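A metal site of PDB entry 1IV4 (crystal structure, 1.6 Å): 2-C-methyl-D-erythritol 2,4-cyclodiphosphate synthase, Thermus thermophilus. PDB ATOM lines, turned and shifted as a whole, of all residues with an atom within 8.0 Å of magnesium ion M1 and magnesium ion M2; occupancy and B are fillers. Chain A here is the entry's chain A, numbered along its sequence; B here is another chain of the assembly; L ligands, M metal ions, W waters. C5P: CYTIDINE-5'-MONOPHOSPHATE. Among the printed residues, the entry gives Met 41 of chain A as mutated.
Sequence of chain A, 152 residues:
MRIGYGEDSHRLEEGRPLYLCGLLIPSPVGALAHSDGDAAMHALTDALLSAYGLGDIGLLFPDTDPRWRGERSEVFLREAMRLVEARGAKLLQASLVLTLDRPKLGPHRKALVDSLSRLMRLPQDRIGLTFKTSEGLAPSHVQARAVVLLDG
N of Thr 133 of chain B sits at hydrogen-bond distance from O3P of the ligand, 2.6 Å away.
The side-chain hydroxyl of Thr 133 of chain B sits at hydrogen-bond distance from an oxygen (O3P) of the ligand, 2.6 Å away.
N of Gly 58 sits at hydrogen-bond distance from O3' of the ligand (2.9 Å).
Two residues have an atom within 4 Å of magnesium ion M2: Asp 8 and Lys 132 of chain B.
The nearest printed residue that does not touch magnesium ion M2 is Ser 9 (4.02 Å).
Magnesium ion M1 is bound by water W3 (1.9 Å), ND1 of His 42 (1.9 Å), OD2 of Asp 8 (2.0 Å) and NE2 of His 10 (2.1 Å).
Slightly farther from magnesium ion M1 lies the side-chain carboxylate (OD1) of Asp 8 (2.8 Å).
The side-chain hydroxyl (OG) of Ser 73 is in hydrogen-bond range of a ring nitrogen (NE2) of His 42.
The backbone NH (N) of His 10 lies within hydrogen-bond range of the backbone carbonyl oxygen (O) of Val 142, 2.9 Å away.
Water W1 lies within hydrogen-bond range of O of Ser 9 (2.5 Å), OE1 of Glu 135 of chain B (2.9 Å) and ND1 of His 10 (3.2 Å).
Water W2 binds magnesium ion M2 (2.0 Å).
The side-chain amino group (NZ) of Lys 132 of chain B is bound to magnesium ion M2, at 2.1 Å.
OD1 of Asp 8 binds magnesium ion M2, at 2.1 Å.
An oxygen (O2P) of the ligand is bound to magnesium ion M2, at 2.2 Å.
Water W3 binds magnesium ion M2 (2.2 Å).
Water W1 is bound to magnesium ion M2.
Magnesium ion M2 has six donor atoms within binding distance.
Of the 25 residues printed, 3 come within 4 Å of magnesium ion M1.
The nearest printed residue that does not touch magnesium ion M1 is Lys 132 of chain B (4.4 Å).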
ATOM      1  N   GLU A   7       2.426 -24.419  20.651  1.00  0.00           N
ATOM      2  CA  GLU A   7       3.172 -23.385  21.383  1.00  0.00           C
ATOM      3  C   GLU A   7       3.860 -22.439  20.391  1.00  0.00           C
ATOM      4  O   GLU A   7       4.149 -22.852  19.265  1.00  0.00           O
ATOM      5  CB  GLU A   7       4.262 -24.008  22.241  1.00  0.00           C
ATOM      6  CG  GLU A   7       3.813 -24.918  23.382  1.00  0.00           C
ATOM      7  CD  GLU A   7       5.012 -25.256  24.264  1.00  0.00           C
ATOM      8  OE1 GLU A   7       5.813 -24.316  24.564  1.00  0.00           O
ATOM      9  OE2 GLU A   7       5.162 -26.398  24.711  1.00  0.00           O
ATOM     10  N   ASP A   8       4.138 -21.222  20.801  1.00  0.00           N
ATOM     11  CA  ASP A   8       5.016 -20.322  20.028  1.00  0.00           C
ATOM     12  C   ASP A   8       5.707 -19.392  20.998  1.00  0.00           C
ATOM     13  O   ASP A   8       5.240 -19.150  22.098  1.00  0.00           O
ATOM     14  CB  ASP A   8       4.267 -19.538  18.955  1.00  0.00           C
ATOM     15  CG  ASP A   8       5.219 -18.921  17.920  1.00  0.00           C
ATOM     16  OD1 ASP A   8       6.380 -19.354  17.832  1.00  0.00           O
ATOM     17  OD2 ASP A   8       4.850 -17.809  17.455  1.00  0.00           O
ATOM     18  N   SER A   9       6.860 -18.863  20.600  1.00  0.00           N
ATOM     19  CA  SER A   9       7.461 -17.771  21.361  1.00  0.00           C
ATOM     20  C   SER A   9       8.212 -16.869  20.383  1.00  0.00           C
ATOM     21  O   SER A   9       8.604 -17.288  19.297  1.00  0.00           O
ATOM     22  CB  SER A   9       8.382 -18.277  22.451  1.00  0.00           C
ATOM     23  OG  SER A   9       9.492 -18.963  21.922  1.00  0.00           O
ATOM     24  N   HIS A  10       8.387 -15.633  20.827  1.00  0.00           N
ATOM     25  CA  HIS A  10       9.166 -14.686  20.039  1.00  0.00           C
ATOM     26  C   HIS A  10       9.947 -13.787  20.983  1.00  0.00           C
ATOM     27  O   HIS A  10       9.417 -13.370  22.002  1.00  0.00           O
ATOM     28  CB  HIS A  10       8.291 -13.843  19.116  1.00  0.00           C
ATOM     29  CG  HIS A  10       7.778 -14.570  17.923  1.00  0.00           C
ATOM     30  ND1 HIS A  10       8.545 -14.783  16.798  1.00  0.00           N
ATOM     31  CD2 HIS A  10       6.572 -15.135  17.655  1.00  0.00           C
ATOM     32  CE1 HIS A  10       7.836 -15.457  15.895  1.00  0.00           C
ATOM     33  NE2 HIS A  10       6.641 -15.686  16.393  1.00  0.00           N
ATOM     34  N   ALA A  31       7.554  -8.071  18.389  1.00  0.00           N
ATOM     35  CA  ALA A  31       8.310  -9.249  18.007  1.00  0.00           C
ATOM     36  C   ALA A  31       9.451  -8.872  17.059  1.00  0.00           C
ATOM     37  O   ALA A  31       9.233  -8.072  16.146  1.00  0.00           O
ATOM     38  CB  ALA A  31       7.412 -10.304  17.371  1.00  0.00           C
ATOM     39  N   ALA A  33      11.029 -10.558  14.365  1.00  0.00           N
ATOM     40  CA  ALA A  33      10.760 -11.790  13.611  1.00  0.00           C
ATOM     41  C   ALA A  33      10.695 -11.531  12.114  1.00  0.00           C
ATOM     42  O   ALA A  33      10.610 -10.376  11.674  1.00  0.00           O
ATOM     43  CB  ALA A  33       9.458 -12.433  14.080  1.00  0.00           C
ATOM     44  N   SER A  35       8.324 -12.837  10.608  1.00  0.00           N
ATOM     45  CA  SER A  35       6.866 -12.826  10.574  1.00  0.00           C
ATOM     46  C   SER A  35       6.345 -11.592  11.302  1.00  0.00           C
ATOM     47  O   SER A  35       7.157 -10.735  11.669  1.00  0.00           O
ATOM     48  CB  SER A  35       6.308 -14.106  11.201  1.00  0.00           C
ATOM     49  OG  SER A  35       6.774 -14.270  12.533  1.00  0.00           O
ATOM     50  N   ASP A  36       5.037 -11.524  11.514  1.00  0.00           N
ATOM     51  CA  ASP A  36       4.491 -10.501  12.400  1.00  0.00           C
ATOM     52  C   ASP A  36       4.728 -10.893  13.866  1.00  0.00           C
ATOM     53  O   ASP A  36       4.476 -10.120  14.794  1.00  0.00           O
ATOM     54  CB  ASP A  36       3.019 -10.236  12.131  1.00  0.00           C
ATOM     55  CG  ASP A  36       2.124 -11.454  12.266  1.00  0.00           C
ATOM     56  OD1 ASP A  36       0.962 -11.367  11.808  1.00  0.00           O
ATOM     57  OD2 ASP A  36       2.596 -12.449  12.857  1.00  0.00           O
ATOM     58  N   GLY A  37       5.226 -12.116  14.065  1.00  0.00           N
ATOM     59  CA  GLY A  37       5.558 -12.577  15.388  1.00  0.00           C
ATOM     60  C   GLY A  37       4.357 -12.731  16.293  1.00  0.00           C
ATOM     61  O   GLY A  37       4.484 -12.657  17.503  1.00  0.00           O
ATOM     62  N   ASP A  38       3.176 -12.936  15.717  1.00  0.00           N
ATOM     63  CA  ASP A  38       1.992 -13.125  16.561  1.00  0.00           C
ATOM     64  C   ASP A  38       1.960 -14.518  17.216  1.00  0.00           C
ATOM     65  O   ASP A  38       1.527 -15.493  16.564  1.00  0.00           O
ATOM     66  CB  ASP A  38       0.743 -12.897  15.722  1.00  0.00           C
ATOM     67  CG  ASP A  38      -0.550 -12.792  16.503  1.00  0.00           C
ATOM     68  OD1 ASP A  38      -0.709 -13.495  17.528  1.00  0.00           O
ATOM     69  OD2 ASP A  38      -1.438 -12.025  16.059  1.00  0.00           O
ATOM     70  N   ALA A  39       2.405 -14.590  18.452  1.00  0.00           N
ATOM     71  CA  ALA A  39       2.559 -15.886  19.130  1.00  0.00           C
ATOM     72  C   ALA A  39       1.231 -16.607  19.354  1.00  0.00           C
ATOM     73  O   ALA A  39       1.158 -17.846  19.347  1.00  0.00           O
ATOM     74  CB  ALA A  39       3.205 -15.709  20.494  1.00  0.00           C
ATOM     75  N   ALA A  40       0.200 -15.789  19.573  1.00  0.00           N
ATOM     76  CA  ALA A  40      -1.148 -16.350  19.770  1.00  0.00           C
ATOM     77  C   ALA A  40      -1.619 -17.029  18.495  1.00  0.00           C
ATOM     78  O   ALA A  40      -2.066 -18.181  18.502  1.00  0.00           O
ATOM     79  CB  ALA A  40      -2.186 -15.296  20.153  1.00  0.00           C
ATOM     80  N   MET A  41      -1.509 -16.330  17.370  1.00  0.00           N
ATOM     81  CA  MET A  41      -1.909 -16.903  16.085  1.00  0.00           C
ATOM     82  C   MET A  41      -1.090 -18.088  15.864  1.00  0.00           C
ATOM     83  O   MET A  41      -1.612 -19.187  15.351  1.00  0.00           O
ATOM     84  CB  MET A  41      -1.655 -15.977  14.941  1.00  0.00           C
ATOM     85  CG  MET A  41      -2.741 -14.924  14.840  1.00  0.00           C
ATOM     86  SD  MET A  41      -4.317 -15.573  14.395  1.00  0.00           S
ATOM     87  CE  MET A  41      -5.471 -15.273  15.709  1.00  0.00           C
ATOM     88  N   HIS A  42       0.235 -18.067  16.013  1.00  0.00           N
ATOM     89  CA  HIS A  42       1.048 -19.238  15.666  1.00  0.00           C
ATOM     90  C   HIS A  42       0.723 -20.456  16.509  1.00  0.00           C
ATOM     91  O   HIS A  42       0.585 -21.593  16.005  1.00  0.00           O
ATOM     92  CB  HIS A  42       2.519 -18.863  15.809  1.00  0.00           C
ATOM     93  CG  HIS A  42       2.941 -17.863  14.781  1.00  0.00           C
ATOM     94  ND1 HIS A  42       4.175 -17.282  14.769  1.00  0.00           N
ATOM     95  CD2 HIS A  42       2.266 -17.380  13.720  1.00  0.00           C
ATOM     96  CE1 HIS A  42       4.268 -16.449  13.742  1.00  0.00           C
ATOM     97  NE2 HIS A  42       3.121 -16.484  13.093  1.00  0.00           N
ATOM     98  N   ALA A  43       0.605 -20.251  17.833  1.00  0.00           N
ATOM     99  CA  ALA A  43       0.299 -21.393  18.708  1.00  0.00           C
ATOM    100  C   ALA A  43      -1.036 -22.046  18.346  1.00  0.00           C
ATOM    101  O   ALA A  43      -1.175 -23.267  18.301  1.00  0.00           O
ATOM    102  CB  ALA A  43       0.305 -20.989  20.180  1.00  0.00           C
ATOM    103  N   ASP A  46      -0.583 -24.027  15.018  1.00  0.00           N
ATOM    104  CA  ASP A  46       0.059 -25.303  15.249  1.00  0.00           C
ATOM    105  C   ASP A  46      -0.882 -26.251  15.986  1.00  0.00           C
ATOM    106  O   ASP A  46      -0.876 -27.449  15.668  1.00  0.00           O
ATOM    107  CB  ASP A  46       1.357 -25.173  16.076  1.00  0.00           C
ATOM    108  CG  ASP A  46       2.589 -24.939  15.207  1.00  0.00           C
ATOM    109  OD1 ASP A  46       2.446 -25.017  13.960  1.00  0.00           O
ATOM    110  OD2 ASP A  46       3.639 -24.699  15.824  1.00  0.00           O
ATOM    111  N   ILE A  57       3.673 -25.011  11.496  1.00  0.00           N
ATOM    112  CA  ILE A  57       3.651 -23.837  10.621  1.00  0.00           C
ATOM    113  C   ILE A  57       4.942 -23.719   9.820  1.00  0.00           C
ATOM    114  O   ILE A  57       4.908 -23.139   8.713  1.00  0.00           O
ATOM    115  CB  ILE A  57       3.415 -22.570  11.468  1.00  0.00           C
ATOM    116  CG1 ILE A  57       4.383 -22.423  12.631  1.00  0.00           C
ATOM    117  CG2 ILE A  57       1.956 -22.568  11.949  1.00  0.00           C
ATOM    118  CD1 ILE A  57       4.250 -21.038  13.269  1.00  0.00           C
ATOM    119  N   GLY A  58       6.065 -24.216  10.300  1.00  0.00           N
ATOM    120  CA  GLY A  58       7.301 -24.158   9.540  1.00  0.00           C
ATOM    121  C   GLY A  58       7.303 -25.096   8.345  1.00  0.00           C
ATOM    122  O   GLY A  58       7.964 -24.866   7.320  1.00  0.00           O
ATOM    123  N   SER A  73      -0.346 -13.380  10.064  1.00  0.00           N
ATOM    124  CA  SER A  73      -0.521 -14.725  10.651  1.00  0.00           C
ATOM    125  C   SER A  73      -1.945 -15.217  10.606  1.00  0.00           C
ATOM    126  O   SER A  73      -2.153 -16.448  10.640  1.00  0.00           O
ATOM    127  CB  SER A  73       0.055 -14.678  12.068  1.00  0.00           C
ATOM    128  OG  SER A  73       1.432 -14.338  11.970  1.00  0.00           O
ATOM    129  N   VAL A 142       7.670 -13.056  24.267  1.00  0.00           N
ATOM    130  CA  VAL A 142       6.237 -13.339  24.361  1.00  0.00           C
ATOM    131  C   VAL A 142       6.100 -14.843  24.088  1.00  0.00           C
ATOM    132  O   VAL A 142       6.731 -15.325  23.140  1.00  0.00           O
ATOM    133  CB  VAL A 142       5.387 -12.484  23.423  1.00  0.00           C
ATOM    134  CG1 VAL A 142       5.799 -12.553  21.948  1.00  0.00           C
ATOM    135  CG2 VAL A 142       3.919 -12.844  23.591  1.00  0.00           C
ATOM    136  N   PHE B 131       7.268 -28.891  16.097  1.00  0.00           N
ATOM    137  CA  PHE B 131       8.580 -28.498  16.587  1.00  0.00           C
ATOM    138  C   PHE B 131       8.758 -26.985  16.703  1.00  0.00           C
ATOM    139  O   PHE B 131       8.233 -26.313  15.818  1.00  0.00           O
ATOM    140  CB  PHE B 131       9.699 -28.938  15.626  1.00  0.00           C
ATOM    141  CG  PHE B 131       9.559 -30.369  15.171  1.00  0.00           C
ATOM    142  CD1 PHE B 131       9.407 -31.383  16.094  1.00  0.00           C
ATOM    143  CD2 PHE B 131       9.584 -30.676  13.823  1.00  0.00           C
ATOM    144  CE1 PHE B 131       9.235 -32.684  15.677  1.00  0.00           C
ATOM    145  CE2 PHE B 131       9.395 -31.976  13.405  1.00  0.00           C
ATOM    146  CZ  PHE B 131       9.225 -32.987  14.327  1.00  0.00           C
ATOM    147  N   LYS B 132       9.492 -26.547  17.729  1.00  0.00           N
ATOM    148  CA  LYS B 132       9.853 -25.130  17.762  1.00  0.00           C
ATOM    149  C   LYS B 132      11.252 -24.951  18.336  1.00  0.00           C
ATOM    150  O   LYS B 132      11.752 -25.833  19.044  1.00  0.00           O
ATOM    151  CB  LYS B 132       8.882 -24.274  18.581  1.00  0.00           C
ATOM    152  CG  LYS B 132       7.418 -24.593  18.607  1.00  0.00           C
ATOM    153  CD  LYS B 132       6.528 -23.771  17.703  1.00  0.00           C
ATOM    154  CE  LYS B 132       6.910 -22.327  17.546  1.00  0.00           C
ATOM    155  NZ  LYS B 132       6.698 -21.756  16.170  1.00  0.00           N
ATOM    156  N   THR B 133      11.840 -23.787  18.000  1.00  0.00           N
ATOM    157  CA  THR B 133      13.068 -23.394  18.699  1.00  0.00           C
ATOM    158  C   THR B 133      12.677 -22.670  19.977  1.00  0.00           C
ATOM    159  O   THR B 133      11.490 -22.461  20.223  1.00  0.00           O
ATOM    160  CB  THR B 133      14.003 -22.465  17.917  1.00  0.00           C
ATOM    161  OG1 THR B 133      13.358 -21.203  17.710  1.00  0.00           O
ATOM    162  CG2 THR B 133      14.259 -23.033  16.530  1.00  0.00           C
ATOM    163  N   SER B 134      13.681 -22.289  20.761  1.00  0.00           N
ATOM    164  CA  SER B 134      13.386 -21.640  22.027  1.00  0.00           C
ATOM    165  C   SER B 134      13.549 -20.126  21.864  1.00  0.00           C
ATOM    166  O   SER B 134      13.347 -19.412  22.862  1.00  0.00           O
ATOM    167  CB  SER B 134      14.242 -22.134  23.185  1.00  0.00           C
ATOM    168  OG  SER B 134      15.603 -21.760  23.148  1.00  0.00           O
ATOM    169  N   GLU B 135      13.908 -19.752  20.646  1.00  0.00           N
ATOM    170  CA  GLU B 135      14.191 -18.353  20.332  1.00  0.00           C
ATOM    171  C   GLU B 135      15.150 -17.786  21.371  1.00  0.00           C
ATOM    172  O   GLU B 135      14.973 -16.666  21.838  1.00  0.00           O
ATOM    173  CB  GLU B 135      12.915 -17.515  20.268  1.00  0.00           C
ATOM    174  CG  GLU B 135      11.973 -17.816  19.129  1.00  0.00           C
ATOM    175  CD  GLU B 135      12.495 -17.581  17.739  1.00  0.00           C
ATOM    176  OE1 GLU B 135      11.837 -18.001  16.749  1.00  0.00           O
ATOM    177  OE2 GLU B 135      13.586 -16.970  17.596  1.00  0.00           O
HETATM  178  O3P C5P L   1      10.998 -21.675  16.646  1.00  0.00           O
HETATM  179  P   C5P L   1      10.714 -21.191  15.174  1.00  0.00           P
HETATM  180  O1P C5P L   1      11.871 -20.540  14.585  1.00  0.00           O
HETATM  181  O2P C5P L   1       9.276 -20.651  14.880  1.00  0.00           O
HETATM  182  O5' C5P L   1      10.521 -22.548  14.308  1.00  0.00           O
HETATM  183  C5' C5P L   1      10.178 -22.476  12.956  1.00  0.00           C
HETATM  184  C4' C5P L   1      10.122 -23.853  12.479  1.00  0.00           C
HETATM  185  O4' C5P L   1      11.251 -24.746  12.392  1.00  0.00           O
HETATM  186  C3' C5P L   1       8.942 -24.719  12.997  1.00  0.00           C
HETATM  187  O3' C5P L   1       7.589 -24.271  12.780  1.00  0.00           O
HETATM  188  C2' C5P L   1       9.394 -26.135  12.843  1.00  0.00           C
HETATM  189  O2' C5P L   1       8.990 -26.364  11.531  1.00  0.00           O
HETATM  190  C1' C5P L   1      10.795 -26.073  12.371  1.00  0.00           C
HETATM  191  N1  C5P L   1      11.734 -26.520  13.517  1.00  0.00           N
HETATM  192  C2  C5P L   1      12.444 -27.779  13.322  1.00  0.00           C
HETATM  193  N3  C5P L   1      13.285 -28.277  14.249  1.00  0.00           N
HETATM  194  C4  C5P L   1      13.525 -27.589  15.471  1.00  0.00           C
HETATM  195  C5  C5P L   1      12.870 -26.334  15.762  1.00  0.00           C
HETATM  196  C6  C5P L   1      12.001 -25.888  14.774  1.00  0.00           C
HETATM  197  O2  C5P L   1      12.248 -28.400  12.247  1.00  0.00           O
HETATM  198  N4  C5P L   1      14.386 -28.073  16.376  1.00  0.00           N
HETATM  199 MG    MG M   1       5.825 -17.514  15.742  1.00  0.00          MG
HETATM  200 MG    MG M   2       7.859 -20.009  16.430  1.00  0.00          MG
HETATM  201  O   HOH W   1       8.982 -17.990  16.916  1.00  0.00           O
HETATM  202  O   HOH W   2       9.040 -20.603  17.988  1.00  0.00           O
HETATM  203  O   HOH W   3       6.725 -18.936  14.852  1.00  0.00           O
